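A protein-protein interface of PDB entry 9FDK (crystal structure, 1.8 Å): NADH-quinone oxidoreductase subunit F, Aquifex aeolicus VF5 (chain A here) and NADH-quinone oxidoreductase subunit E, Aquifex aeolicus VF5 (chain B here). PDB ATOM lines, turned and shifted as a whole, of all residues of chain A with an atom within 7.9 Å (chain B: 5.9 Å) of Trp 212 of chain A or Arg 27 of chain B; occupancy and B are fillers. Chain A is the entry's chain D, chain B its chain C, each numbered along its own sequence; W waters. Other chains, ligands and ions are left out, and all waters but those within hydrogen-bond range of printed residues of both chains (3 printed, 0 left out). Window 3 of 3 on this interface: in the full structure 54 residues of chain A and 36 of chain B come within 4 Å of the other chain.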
ATOM      1  N   PRO A  86     -29.604   7.519   5.129  1.00  0.00           N
ATOM      2  CA  PRO A  86     -28.602   7.562   6.187  1.00  0.00           C
ATOM      3  C   PRO A  86     -28.722   8.803   7.066  1.00  0.00           C
ATOM      4  O   PRO A  86     -29.313   9.808   6.658  1.00  0.00           O
ATOM      5  CB  PRO A  86     -27.260   7.520   5.423  1.00  0.00           C
ATOM      6  CG  PRO A  86     -27.589   8.118   4.082  1.00  0.00           C
ATOM      7  CD  PRO A  86     -29.023   7.679   3.788  1.00  0.00           C
ATOM      8  N   TYR A  88     -26.542  11.398  10.079  1.00  0.00           N
ATOM      9  CA  TYR A  88     -25.234  11.925  10.426  1.00  0.00           C
ATOM     10  C   TYR A  88     -25.290  12.435  11.855  1.00  0.00           C
ATOM     11  O   TYR A  88     -26.334  12.921  12.309  1.00  0.00           O
ATOM     12  CB  TYR A  88     -24.772  13.043   9.489  1.00  0.00           C
ATOM     13  CG  TYR A  88     -24.619  12.590   8.046  1.00  0.00           C
ATOM     14  CD1 TYR A  88     -23.602  11.712   7.689  1.00  0.00           C
ATOM     15  CD2 TYR A  88     -25.475  13.047   7.057  1.00  0.00           C
ATOM     16  CE1 TYR A  88     -23.459  11.273   6.385  1.00  0.00           C
ATOM     17  CE2 TYR A  88     -25.343  12.616   5.747  1.00  0.00           C
ATOM     18  CZ  TYR A  88     -24.324  11.738   5.409  1.00  0.00           C
ATOM     19  OH  TYR A  88     -24.187  11.311   4.120  1.00  0.00           O
ATOM     20  N   GLU A 129     -21.249   7.835   9.977  1.00  0.00           N
ATOM     21  CA  GLU A 129     -20.313   8.915   9.742  1.00  0.00           C
ATOM     22  C   GLU A 129     -20.621  10.007  10.762  1.00  0.00           C
ATOM     23  O   GLU A 129     -21.760  10.466  10.861  1.00  0.00           O
ATOM     24  CB  GLU A 129     -20.458   9.295   8.266  1.00  0.00           C
ATOM     25  CG  GLU A 129     -19.884  10.648   7.849  1.00  0.00           C
ATOM     26  CD  GLU A 129     -19.987  10.937   6.346  1.00  0.00           C
ATOM     27  OE1 GLU A 129     -20.121   9.953   5.601  1.00  0.00           O
ATOM     28  OE2 GLU A 129     -19.965  12.126   5.908  1.00  0.00           O
ATOM     29  N   TYR A 131     -18.953  13.724  12.703  1.00  0.00           N
ATOM     30  CA  TYR A 131     -17.996  14.806  12.564  1.00  0.00           C
ATOM     31  C   TYR A 131     -17.808  15.491  13.905  1.00  0.00           C
ATOM     32  O   TYR A 131     -18.729  15.519  14.717  1.00  0.00           O
ATOM     33  CB  TYR A 131     -18.507  15.877  11.603  1.00  0.00           C
ATOM     34  CG  TYR A 131     -18.598  15.374  10.185  1.00  0.00           C
ATOM     35  CD1 TYR A 131     -19.690  14.628   9.745  1.00  0.00           C
ATOM     36  CD2 TYR A 131     -17.555  15.614   9.305  1.00  0.00           C
ATOM     37  CE1 TYR A 131     -19.749  14.171   8.440  1.00  0.00           C
ATOM     38  CE2 TYR A 131     -17.611  15.175   8.003  1.00  0.00           C
ATOM     39  CZ  TYR A 131     -18.700  14.442   7.573  1.00  0.00           C
ATOM     40  OH  TYR A 131     -18.701  14.029   6.273  1.00  0.00           O
ATOM     41  N   ILE A 189     -23.373  23.099   9.525  1.00  0.00           N
ATOM     42  CA  ILE A 189     -23.577  22.143   8.453  1.00  0.00           C
ATOM     43  C   ILE A 189     -23.158  22.739   7.108  1.00  0.00           C
ATOM     44  O   ILE A 189     -22.476  22.058   6.349  1.00  0.00           O
ATOM     45  CB  ILE A 189     -25.023  21.623   8.452  1.00  0.00           C
ATOM     46  CG1 ILE A 189     -25.293  20.754   9.676  1.00  0.00           C
ATOM     47  CG2 ILE A 189     -25.316  20.891   7.150  1.00  0.00           C
ATOM     48  CD1 ILE A 189     -26.760  20.506   9.974  1.00  0.00           C
ATOM     49  N   GLU A 190     -23.524  24.003   6.823  1.00  0.00           N
ATOM     50  CA  GLU A 190     -23.100  24.663   5.599  1.00  0.00           C
ATOM     51  C   GLU A 190     -21.575  24.665   5.499  1.00  0.00           C
ATOM     52  O   GLU A 190     -21.010  24.406   4.432  1.00  0.00           O
ATOM     53  CB  GLU A 190     -23.625  26.098   5.526  1.00  0.00           C
ATOM     54  CG  GLU A 190     -25.130  26.185   5.272  1.00  0.00           C
ATOM     55  CD  GLU A 190     -25.524  25.717   3.876  1.00  0.00           C
ATOM     56  OE1 GLU A 190     -24.960  26.222   2.880  1.00  0.00           O
ATOM     57  OE2 GLU A 190     -26.376  24.819   3.770  1.00  0.00           O
ATOM     58  N   SER A 191     -20.909  24.928   6.622  1.00  0.00           N
ATOM     59  CA  SER A 191     -19.451  24.967   6.654  1.00  0.00           C
ATOM     60  C   SER A 191     -18.848  23.577   6.407  1.00  0.00           C
ATOM     61  O   SER A 191     -17.898  23.413   5.644  1.00  0.00           O
ATOM     62  CB  SER A 191     -18.994  25.566   7.969  1.00  0.00           C
ATOM     63  OG  SER A 191     -17.601  25.830   7.957  1.00  0.00           O
ATOM     64  N   LEU A 192     -19.461  22.545   6.985  1.00  0.00           N
ATOM     65  CA  LEU A 192     -19.035  21.173   6.765  1.00  0.00           C
ATOM     66  C   LEU A 192     -19.194  20.772   5.301  1.00  0.00           C
ATOM     67  O   LEU A 192     -18.511  19.867   4.834  1.00  0.00           O
ATOM     68  CB  LEU A 192     -19.816  20.206   7.649  1.00  0.00           C
ATOM     69  CG  LEU A 192     -19.270  19.984   9.054  1.00  0.00           C
ATOM     70  CD1 LEU A 192     -20.206  19.050   9.795  1.00  0.00           C
ATOM     71  CD2 LEU A 192     -17.860  19.422   9.002  1.00  0.00           C
ATOM     72  N   GLU A 193     -20.106  21.432   4.583  1.00  0.00           N
ATOM     73  CA  GLU A 193     -20.326  21.163   3.175  1.00  0.00           C
ATOM     74  C   GLU A 193     -19.369  21.995   2.311  1.00  0.00           C
ATOM     75  O   GLU A 193     -19.440  21.943   1.086  1.00  0.00           O
ATOM     76  CB  GLU A 193     -21.792  21.433   2.820  1.00  0.00           C
ATOM     77  CG  GLU A 193     -22.799  20.442   3.409  1.00  0.00           C
ATOM     78  CD  GLU A 193     -24.278  20.736   3.151  1.00  0.00           C
ATOM     79  OE1 GLU A 193     -24.585  21.784   2.534  1.00  0.00           O
ATOM     80  OE2 GLU A 193     -25.142  19.922   3.542  1.00  0.00           O
ATOM     81  N   GLY A 194     -18.509  22.804   2.928  1.00  0.00           N
ATOM     82  CA  GLY A 194     -17.495  23.524   2.175  1.00  0.00           C
ATOM     83  C   GLY A 194     -17.928  24.920   1.740  1.00  0.00           C
ATOM     84  O   GLY A 194     -17.305  25.498   0.860  1.00  0.00           O
ATOM     85  N   LYS A 195     -18.938  25.478   2.412  1.00  0.00           N
ATOM     86  CA  LYS A 195     -19.488  26.774   2.053  1.00  0.00           C
ATOM     87  C   LYS A 195     -19.244  27.777   3.171  1.00  0.00           C
ATOM     88  O   LYS A 195     -18.719  27.449   4.237  1.00  0.00           O
ATOM     89  CB  LYS A 195     -20.979  26.614   1.737  1.00  0.00           C
ATOM     90  CG  LYS A 195     -21.217  25.878   0.429  1.00  0.00           C
ATOM     91  CD  LYS A 195     -22.670  25.528   0.148  1.00  0.00           C
ATOM     92  CE  LYS A 195     -23.096  24.436   1.062  1.00  0.00           C
ATOM     93  NZ  LYS A 195     -24.390  23.864   0.680  1.00  0.00           N
ATOM     94  N   ARG A 200     -29.497  28.470   7.705  1.00  0.00           N
ATOM     95  CA  ARG A 200     -30.627  28.174   6.837  1.00  0.00           C
ATOM     96  C   ARG A 200     -31.925  28.526   7.565  1.00  0.00           C
ATOM     97  O   ARG A 200     -32.022  28.429   8.792  1.00  0.00           O
ATOM     98  CB  ARG A 200     -30.650  26.680   6.496  1.00  0.00           C
ATOM     99  CG  ARG A 200     -29.366  26.083   5.941  1.00  0.00           C
ATOM    100  CD  ARG A 200     -29.542  24.559   5.848  1.00  0.00           C
ATOM    101  NE  ARG A 200     -28.410  23.867   5.234  1.00  0.00           N
ATOM    102  CZ  ARG A 200     -28.256  22.538   5.107  1.00  0.00           C
ATOM    103  NH1 ARG A 200     -29.115  21.691   5.659  1.00  0.00           N
ATOM    104  NH2 ARG A 200     -27.216  22.070   4.423  1.00  0.00           N
ATOM    105  N   LYS A 209     -33.616  17.474   7.787  1.00  0.00           N
ATOM    106  CA  LYS A 209     -32.782  17.714   6.619  1.00  0.00           C
ATOM    107  C   LYS A 209     -31.577  18.536   7.042  1.00  0.00           C
ATOM    108  O   LYS A 209     -31.705  19.733   7.300  1.00  0.00           O
ATOM    109  CB  LYS A 209     -33.500  18.499   5.518  1.00  0.00           C
ATOM    110  CG  LYS A 209     -34.640  17.769   4.833  1.00  0.00           C
ATOM    111  CD  LYS A 209     -35.155  18.456   3.574  1.00  0.00           C
ATOM    112  CE  LYS A 209     -34.180  18.404   2.423  1.00  0.00           C
ATOM    113  NZ  LYS A 209     -33.778  17.031   2.086  1.00  0.00           N
ATOM    114  N   GLY A 210     -30.417  17.884   7.103  1.00  0.00           N
ATOM    115  CA  GLY A 210     -29.194  18.483   7.608  1.00  0.00           C
ATOM    116  C   GLY A 210     -28.062  18.388   6.585  1.00  0.00           C
ATOM    117  O   GLY A 210     -28.146  18.981   5.515  1.00  0.00           O
ATOM    118  N   LEU A 211     -27.014  17.636   6.944  1.00  0.00           N
ATOM    119  CA  LEU A 211     -25.830  17.462   6.117  1.00  0.00           C
ATOM    120  C   LEU A 211     -26.212  16.665   4.882  1.00  0.00           C
ATOM    121  O   LEU A 211     -26.754  15.576   5.022  1.00  0.00           O
ATOM    122  CB  LEU A 211     -24.739  16.760   6.926  1.00  0.00           C
ATOM    123  CG  LEU A 211     -23.405  16.526   6.209  1.00  0.00           C
ATOM    124  CD1 LEU A 211     -22.708  17.835   5.836  1.00  0.00           C
ATOM    125  CD2 LEU A 211     -22.509  15.667   7.069  1.00  0.00           C
ATOM    126  N   TRP A 212     -25.947  17.239   3.698  1.00  0.00           N
ATOM    127  CA  TRP A 212     -26.354  16.681   2.414  1.00  0.00           C
ATOM    128  C   TRP A 212     -27.859  16.389   2.381  1.00  0.00           C
ATOM    129  O   TRP A 212     -28.303  15.490   1.671  1.00  0.00           O
ATOM    130  CB  TRP A 212     -25.536  15.419   2.090  1.00  0.00           C
ATOM    131  CG  TRP A 212     -24.051  15.603   2.275  1.00  0.00           C
ATOM    132  CD1 TRP A 212     -23.221  14.812   3.013  1.00  0.00           C
ATOM    133  CD2 TRP A 212     -23.211  16.634   1.709  1.00  0.00           C
ATOM    134  NE1 TRP A 212     -21.938  15.288   2.975  1.00  0.00           N
ATOM    135  CE2 TRP A 212     -21.901  16.402   2.178  1.00  0.00           C
ATOM    136  CE3 TRP A 212     -23.433  17.725   0.866  1.00  0.00           C
ATOM    137  CZ2 TRP A 212     -20.827  17.219   1.829  1.00  0.00           C
ATOM    138  CZ3 TRP A 212     -22.369  18.531   0.521  1.00  0.00           C
ATOM    139  CH2 TRP A 212     -21.085  18.282   0.997  1.00  0.00           C
ATOM    140  N   GLY A 213     -28.644  17.150   3.153  1.00  0.00           N
ATOM    141  CA  GLY A 213     -30.094  17.032   3.173  1.00  0.00           C
ATOM    142  C   GLY A 213     -30.606  15.814   3.950  1.00  0.00           C
ATOM    143  O   GLY A 213     -31.786  15.500   3.856  1.00  0.00           O
ATOM    144  N   LYS A 214     -29.735  15.119   4.692  1.00  0.00           N
ATOM    145  CA  LYS A 214     -30.119  13.908   5.410  1.00  0.00           C
ATOM    146  C   LYS A 214     -30.346  14.208   6.889  1.00  0.00           C
ATOM    147  O   LYS A 214     -29.810  15.171   7.429  1.00  0.00           O
ATOM    148  CB  LYS A 214     -29.035  12.828   5.309  1.00  0.00           C
ATOM    149  CG  LYS A 214     -28.623  12.457   3.888  1.00  0.00           C
ATOM    150  CD  LYS A 214     -29.789  11.929   3.080  1.00  0.00           C
ATOM    151  CE  LYS A 214     -29.415  11.639   1.664  1.00  0.00           C
ATOM    152  NZ  LYS A 214     -30.644  11.294   0.953  1.00  0.00           N
ATOM    153  N   PRO A 215     -31.096  13.357   7.622  1.00  0.00           N
ATOM    154  CA  PRO A 215     -31.279  13.572   9.059  1.00  0.00           C
ATOM    155  C   PRO A 215     -29.943  13.669   9.778  1.00  0.00           C
ATOM    156  O   PRO A 215     -29.091  12.796   9.643  1.00  0.00           O
ATOM    157  CB  PRO A 215     -32.087  12.358   9.490  1.00  0.00           C
ATOM    158  CG  PRO A 215     -32.802  11.946   8.233  1.00  0.00           C
ATOM    159  CD  PRO A 215     -31.799  12.173   7.122  1.00  0.00           C
ATOM    160  N   THR A 216     -29.782  14.743  10.552  1.00  0.00           N
ATOM    161  CA  THR A 216     -28.522  15.064  11.185  1.00  0.00           C
ATOM    162  C   THR A 216     -28.774  15.504  12.628  1.00  0.00           C
ATOM    163  O   THR A 216     -29.533  16.439  12.868  1.00  0.00           O
ATOM    164  CB  THR A 216     -27.844  16.176  10.379  1.00  0.00           C
ATOM    165  OG1 THR A 216     -27.639  15.705   9.046  1.00  0.00           O
ATOM    166  CG2 THR A 216     -26.520  16.586  10.990  1.00  0.00           C
ATOM    167  N   LYS B  25     -16.181  13.901   0.641  1.00  0.00           N
ATOM    168  CA  LYS B  25     -16.269  14.767  -0.524  1.00  0.00           C
ATOM    169  C   LYS B  25     -15.137  15.783  -0.461  1.00  0.00           C
ATOM    170  O   LYS B  25     -14.811  16.288   0.612  1.00  0.00           O
ATOM    171  CB  LYS B  25     -17.641  15.445  -0.602  1.00  0.00           C
ATOM    172  CG  LYS B  25     -18.785  14.450  -0.571  1.00  0.00           C
ATOM    173  CD  LYS B  25     -20.155  15.065  -0.811  1.00  0.00           C
ATOM    174  CE  LYS B  25     -21.242  14.036  -0.830  1.00  0.00           C
ATOM    175  NZ  LYS B  25     -22.514  14.676  -1.176  1.00  0.00           N
ATOM    176  N   LYS B  26     -14.533  16.043  -1.625  1.00  0.00           N
ATOM    177  CA  LYS B  26     -13.351  16.876  -1.720  1.00  0.00           C
ATOM    178  C   LYS B  26     -13.628  18.274  -1.179  1.00  0.00           C
ATOM    179  O   LYS B  26     -12.780  18.868  -0.527  1.00  0.00           O
ATOM    180  CB  LYS B  26     -12.924  17.044  -3.179  1.00  0.00           C
ATOM    181  CG  LYS B  26     -12.434  15.804  -3.885  1.00  0.00           C
ATOM    182  CD  LYS B  26     -11.997  16.132  -5.310  1.00  0.00           C
ATOM    183  CE  LYS B  26     -11.025  15.152  -5.866  1.00  0.00           C
ATOM    184  NZ  LYS B  26     -11.607  13.818  -6.000  1.00  0.00           N
ATOM    185  N   ARG B  27     -14.808  18.815  -1.490  1.00  0.00           N
ATOM    186  CA  ARG B  27     -15.085  20.209  -1.182  1.00  0.00           C
ATOM    187  C   ARG B  27     -15.152  20.450   0.321  1.00  0.00           C
ATOM    188  O   ARG B  27     -15.012  21.590   0.750  1.00  0.00           O
ATOM    189  CB  ARG B  27     -16.357  20.720  -1.860  1.00  0.00           C
ATOM    190  CG  ARG B  27     -17.651  20.008  -1.501  1.00  0.00           C
ATOM    191  CD  ARG B  27     -18.695  20.460  -2.507  1.00  0.00           C
ATOM    192  NE  ARG B  27     -19.991  19.782  -2.400  1.00  0.00           N
ATOM    193  CZ  ARG B  27     -20.328  18.626  -2.940  1.00  0.00           C
ATOM    194  NH1 ARG B  27     -21.580  18.213  -2.860  1.00  0.00           N
ATOM    195  NH2 ARG B  27     -19.445  17.914  -3.599  1.00  0.00           N
ATOM    196  N   GLN B  28     -15.359  19.395   1.120  1.00  0.00           N
ATOM    197  CA  GLN B  28     -15.359  19.553   2.564  1.00  0.00           C
ATOM    198  C   GLN B  28     -13.981  19.957   3.105  1.00  0.00           C
ATOM    199  O   GLN B  28     -13.889  20.482   4.218  1.00  0.00           O
ATOM    200  CB  GLN B  28     -15.833  18.294   3.285  1.00  0.00           C
ATOM    201  CG  GLN B  28     -17.120  17.721   2.722  1.00  0.00           C
ATOM    202  CD  GLN B  28     -17.630  16.569   3.550  1.00  0.00           C
ATOM    203  OE1 GLN B  28     -17.577  15.408   3.140  1.00  0.00           O
ATOM    204  NE2 GLN B  28     -18.158  16.897   4.714  1.00  0.00           N
ATOM    205  N   ALA B  29     -12.913  19.734   2.325  1.00  0.00           N
ATOM    206  CA  ALA B  29     -11.556  20.001   2.779  1.00  0.00           C
ATOM    207  C   ALA B  29     -11.149  21.473   2.633  1.00  0.00           C
ATOM    208  O   ALA B  29     -10.004  21.824   2.910  1.00  0.00           O
ATOM    209  CB  ALA B  29     -10.585  19.108   2.018  1.00  0.00           C
ATOM    210  N   ILE B  30     -12.056  22.352   2.205  1.00  0.00           N
ATOM    211  CA  ILE B  30     -11.654  23.686   1.772  1.00  0.00           C
ATOM    212  C   ILE B  30     -10.972  24.467   2.901  1.00  0.00           C
ATOM    213  O   ILE B  30      -9.970  25.132   2.655  1.00  0.00           O
ATOM    214  CB  ILE B  30     -12.841  24.470   1.187  1.00  0.00           C
ATOM    215  CG1 ILE B  30     -12.398  25.871   0.719  1.00  0.00           C
ATOM    216  CG2 ILE B  30     -14.011  24.542   2.178  1.00  0.00           C
ATOM    217  CD1 ILE B  30     -13.389  26.556  -0.208  1.00  0.00           C
ATOM    218  N   LEU B  31     -11.510  24.421   4.122  1.00  0.00           N
ATOM    219  CA  LEU B  31     -10.941  25.214   5.207  1.00  0.00           C
ATOM    220  C   LEU B  31      -9.604  24.636   5.673  1.00  0.00           C
ATOM    221  O   LEU B  31      -8.679  25.394   5.979  1.00  0.00           O
ATOM    222  CB  LEU B  31     -11.911  25.351   6.375  1.00  0.00           C
ATOM    223  CG  LEU B  31     -13.269  25.975   6.028  1.00  0.00           C
ATOM    224  CD1 LEU B  31     -14.042  26.183   7.317  1.00  0.00           C
ATOM    225  CD2 LEU B  31     -13.155  27.272   5.247  1.00  0.00           C
ATOM    226  N   LEU B  56     -10.227  21.286  -5.598  1.00  0.00           N
ATOM    227  CA  LEU B  56     -11.466  21.030  -4.872  1.00  0.00           C
ATOM    228  C   LEU B  56     -12.632  20.767  -5.827  1.00  0.00           C
ATOM    229  O   LEU B  56     -13.726  20.423  -5.377  1.00  0.00           O
ATOM    230  CB  LEU B  56     -11.769  22.220  -3.965  1.00  0.00           C
ATOM    231  CG  LEU B  56     -10.746  22.516  -2.864  1.00  0.00           C
ATOM    232  CD1 LEU B  56     -10.984  23.895  -2.294  1.00  0.00           C
ATOM    233  CD2 LEU B  56     -10.792  21.475  -1.779  1.00  0.00           C
ATOM    234  N   LEU B  58     -14.195  23.035  -7.388  1.00  0.00           N
ATOM    235  CA  LEU B  58     -15.117  24.114  -7.059  1.00  0.00           C
ATOM    236  C   LEU B  58     -14.851  25.295  -7.988  1.00  0.00           C
ATOM    237  O   LEU B  58     -13.718  25.494  -8.410  1.00  0.00           O
ATOM    238  CB  LEU B  58     -14.905  24.545  -5.610  1.00  0.00           C
ATOM    239  CG  LEU B  58     -15.430  23.611  -4.521  1.00  0.00           C
ATOM    240  CD1 LEU B  58     -15.106  24.210  -3.171  1.00  0.00           C
ATOM    241  CD2 LEU B  58     -16.923  23.394  -4.658  1.00  0.00           C
ATOM    242  N   HIS B  62     -16.476  30.555  -5.698  1.00  0.00           N
ATOM    243  CA  HIS B  62     -16.845  29.897  -4.448  1.00  0.00           C
ATOM    244  C   HIS B  62     -15.692  30.004  -3.450  1.00  0.00           C
ATOM    245  O   HIS B  62     -15.884  30.381  -2.291  1.00  0.00           O
ATOM    246  CB  HIS B  62     -17.246  28.447  -4.746  1.00  0.00           C
ATOM    247  CG  HIS B  62     -17.703  27.638  -3.579  1.00  0.00           C
ATOM    248  ND1 HIS B  62     -17.053  27.565  -2.364  1.00  0.00           N
ATOM    249  CD2 HIS B  62     -18.744  26.808  -3.481  1.00  0.00           C
ATOM    250  CE1 HIS B  62     -17.715  26.756  -1.561  1.00  0.00           C
ATOM    251  NE2 HIS B  62     -18.738  26.278  -2.216  1.00  0.00           N
HETATM  252  O   HOH W   1     -21.419  21.799  -1.053  1.00  0.00           O
HETATM  253  O   HOH W   2     -19.746  13.551   3.609  1.00  0.00           O
HETATM  254  O   HOH W   3     -15.562  22.075   6.763  1.00  0.00           O
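The side-chain amide nitrogen (NE2) of Gln 28 of chain B sits at hydrogen-bond distance from the side-chain hydroxyl (OH) of Tyr 131 of chain A (3.3 Å).
O of Leu 192 of chain A is in hydrogen-bond range of NE2 of Gln 28 of chain B (3.0 Å).
A ring nitrogen (NE2) of His 62 of chain B sits close to the backbone carbonyl oxygen of Gly 194 of chain A, at 3.5 Å.
N of Lys 25 of chain B is in hydrogen-bond range of OE1 of Gln 28 of chain B (3.2 Å).
NZ of Lys 195 of chain A is in salt-bridge range of OE1 of Glu 190 of chain A, at 3.3 Å.
The side-chain carboxylate (OE1) of Glu 193 of chain A is in salt-bridge range of the side-chain amino group (NZ) of Lys 195 of chain A.
NH2 of Arg 200 of chain A is in salt-bridge range of OE2 of Glu 193 of chain A (3.1 Å).
OE2 of Glu 193 of chain A is in hydrogen-bond range of N of Trp 212 of chain A, 2.8 Å away.
Ser 191 of chain A touches Leu 31 of chain B.
Arg 27 of chain B touches Glu 193 of chain A (CG to O, 3.7 Å).
CA of Gly 194 of chain A touches O of Arg 27 of chain B, 3.5 Å away.
Gly 194 of chain A touches Ile 30 of chain B.
NE2 of His 62 of chain B touches CG of Lys 195 of chain A, 3.6 Å away.
Lys 25 of chain B touches Trp 212 of chain A (CD to CZ2, 3.5 Å).
Trp 212 of chain A touches Arg 27 of chain B (CZ3 to NH1, 3.5 Å).
CZ2 of Trp 212 of chain A touches CD of Gln 28 of chain B, 3.7 Å away.
Printed residues of chain B within 4 Å of Gly 194 of chain A: Arg 27 (3.5 Å), Ile 30 (3.6 Å) and His 62 (2.8 Å).
Of chain B, only Lys 25, Arg 27 and Gln 28 come within 4 Å of Trp 212 of chain A.
Arg 27 of chain B touches just these residues of chain A: Glu 193 (3.7 Å), Gly 194 (3.5 Å) and Trp 212 (3.5 Å).
Of the printed residues of chain A, His 62 of chain B touches Gly 194 (2.8 Å) and Lys 195 (3.6 Å).
The nearest printed residue of chain B that does not touch Trp 212 of chain A is Lys 26 of chain B (7.3 Å).
Among the printed residues, no Asp or Glu carboxylate lies within 4 Å of a Lys or Arg side-chain nitrogen of the other chain.
Water W2 lies within hydrogen-bond range of OE2 of Glu 129 of chain A (2.7 Å), NE1 of Trp 212 of chain A (2.9 Å), OE1 of Gln 28 of chain B (2.9 Å) and OH of Tyr 131 of chain A (2.9 Å).
Water W1 bridges the guanidinium group of Arg 27 of chain B and the backbone carbonyl oxygen of Glu 193 of chain A.
Water W3 lies within hydrogen-bond range of O of Ser 191 of chain A (2.9 Å) and O of Gln 28 of chain B (3.4 Å).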
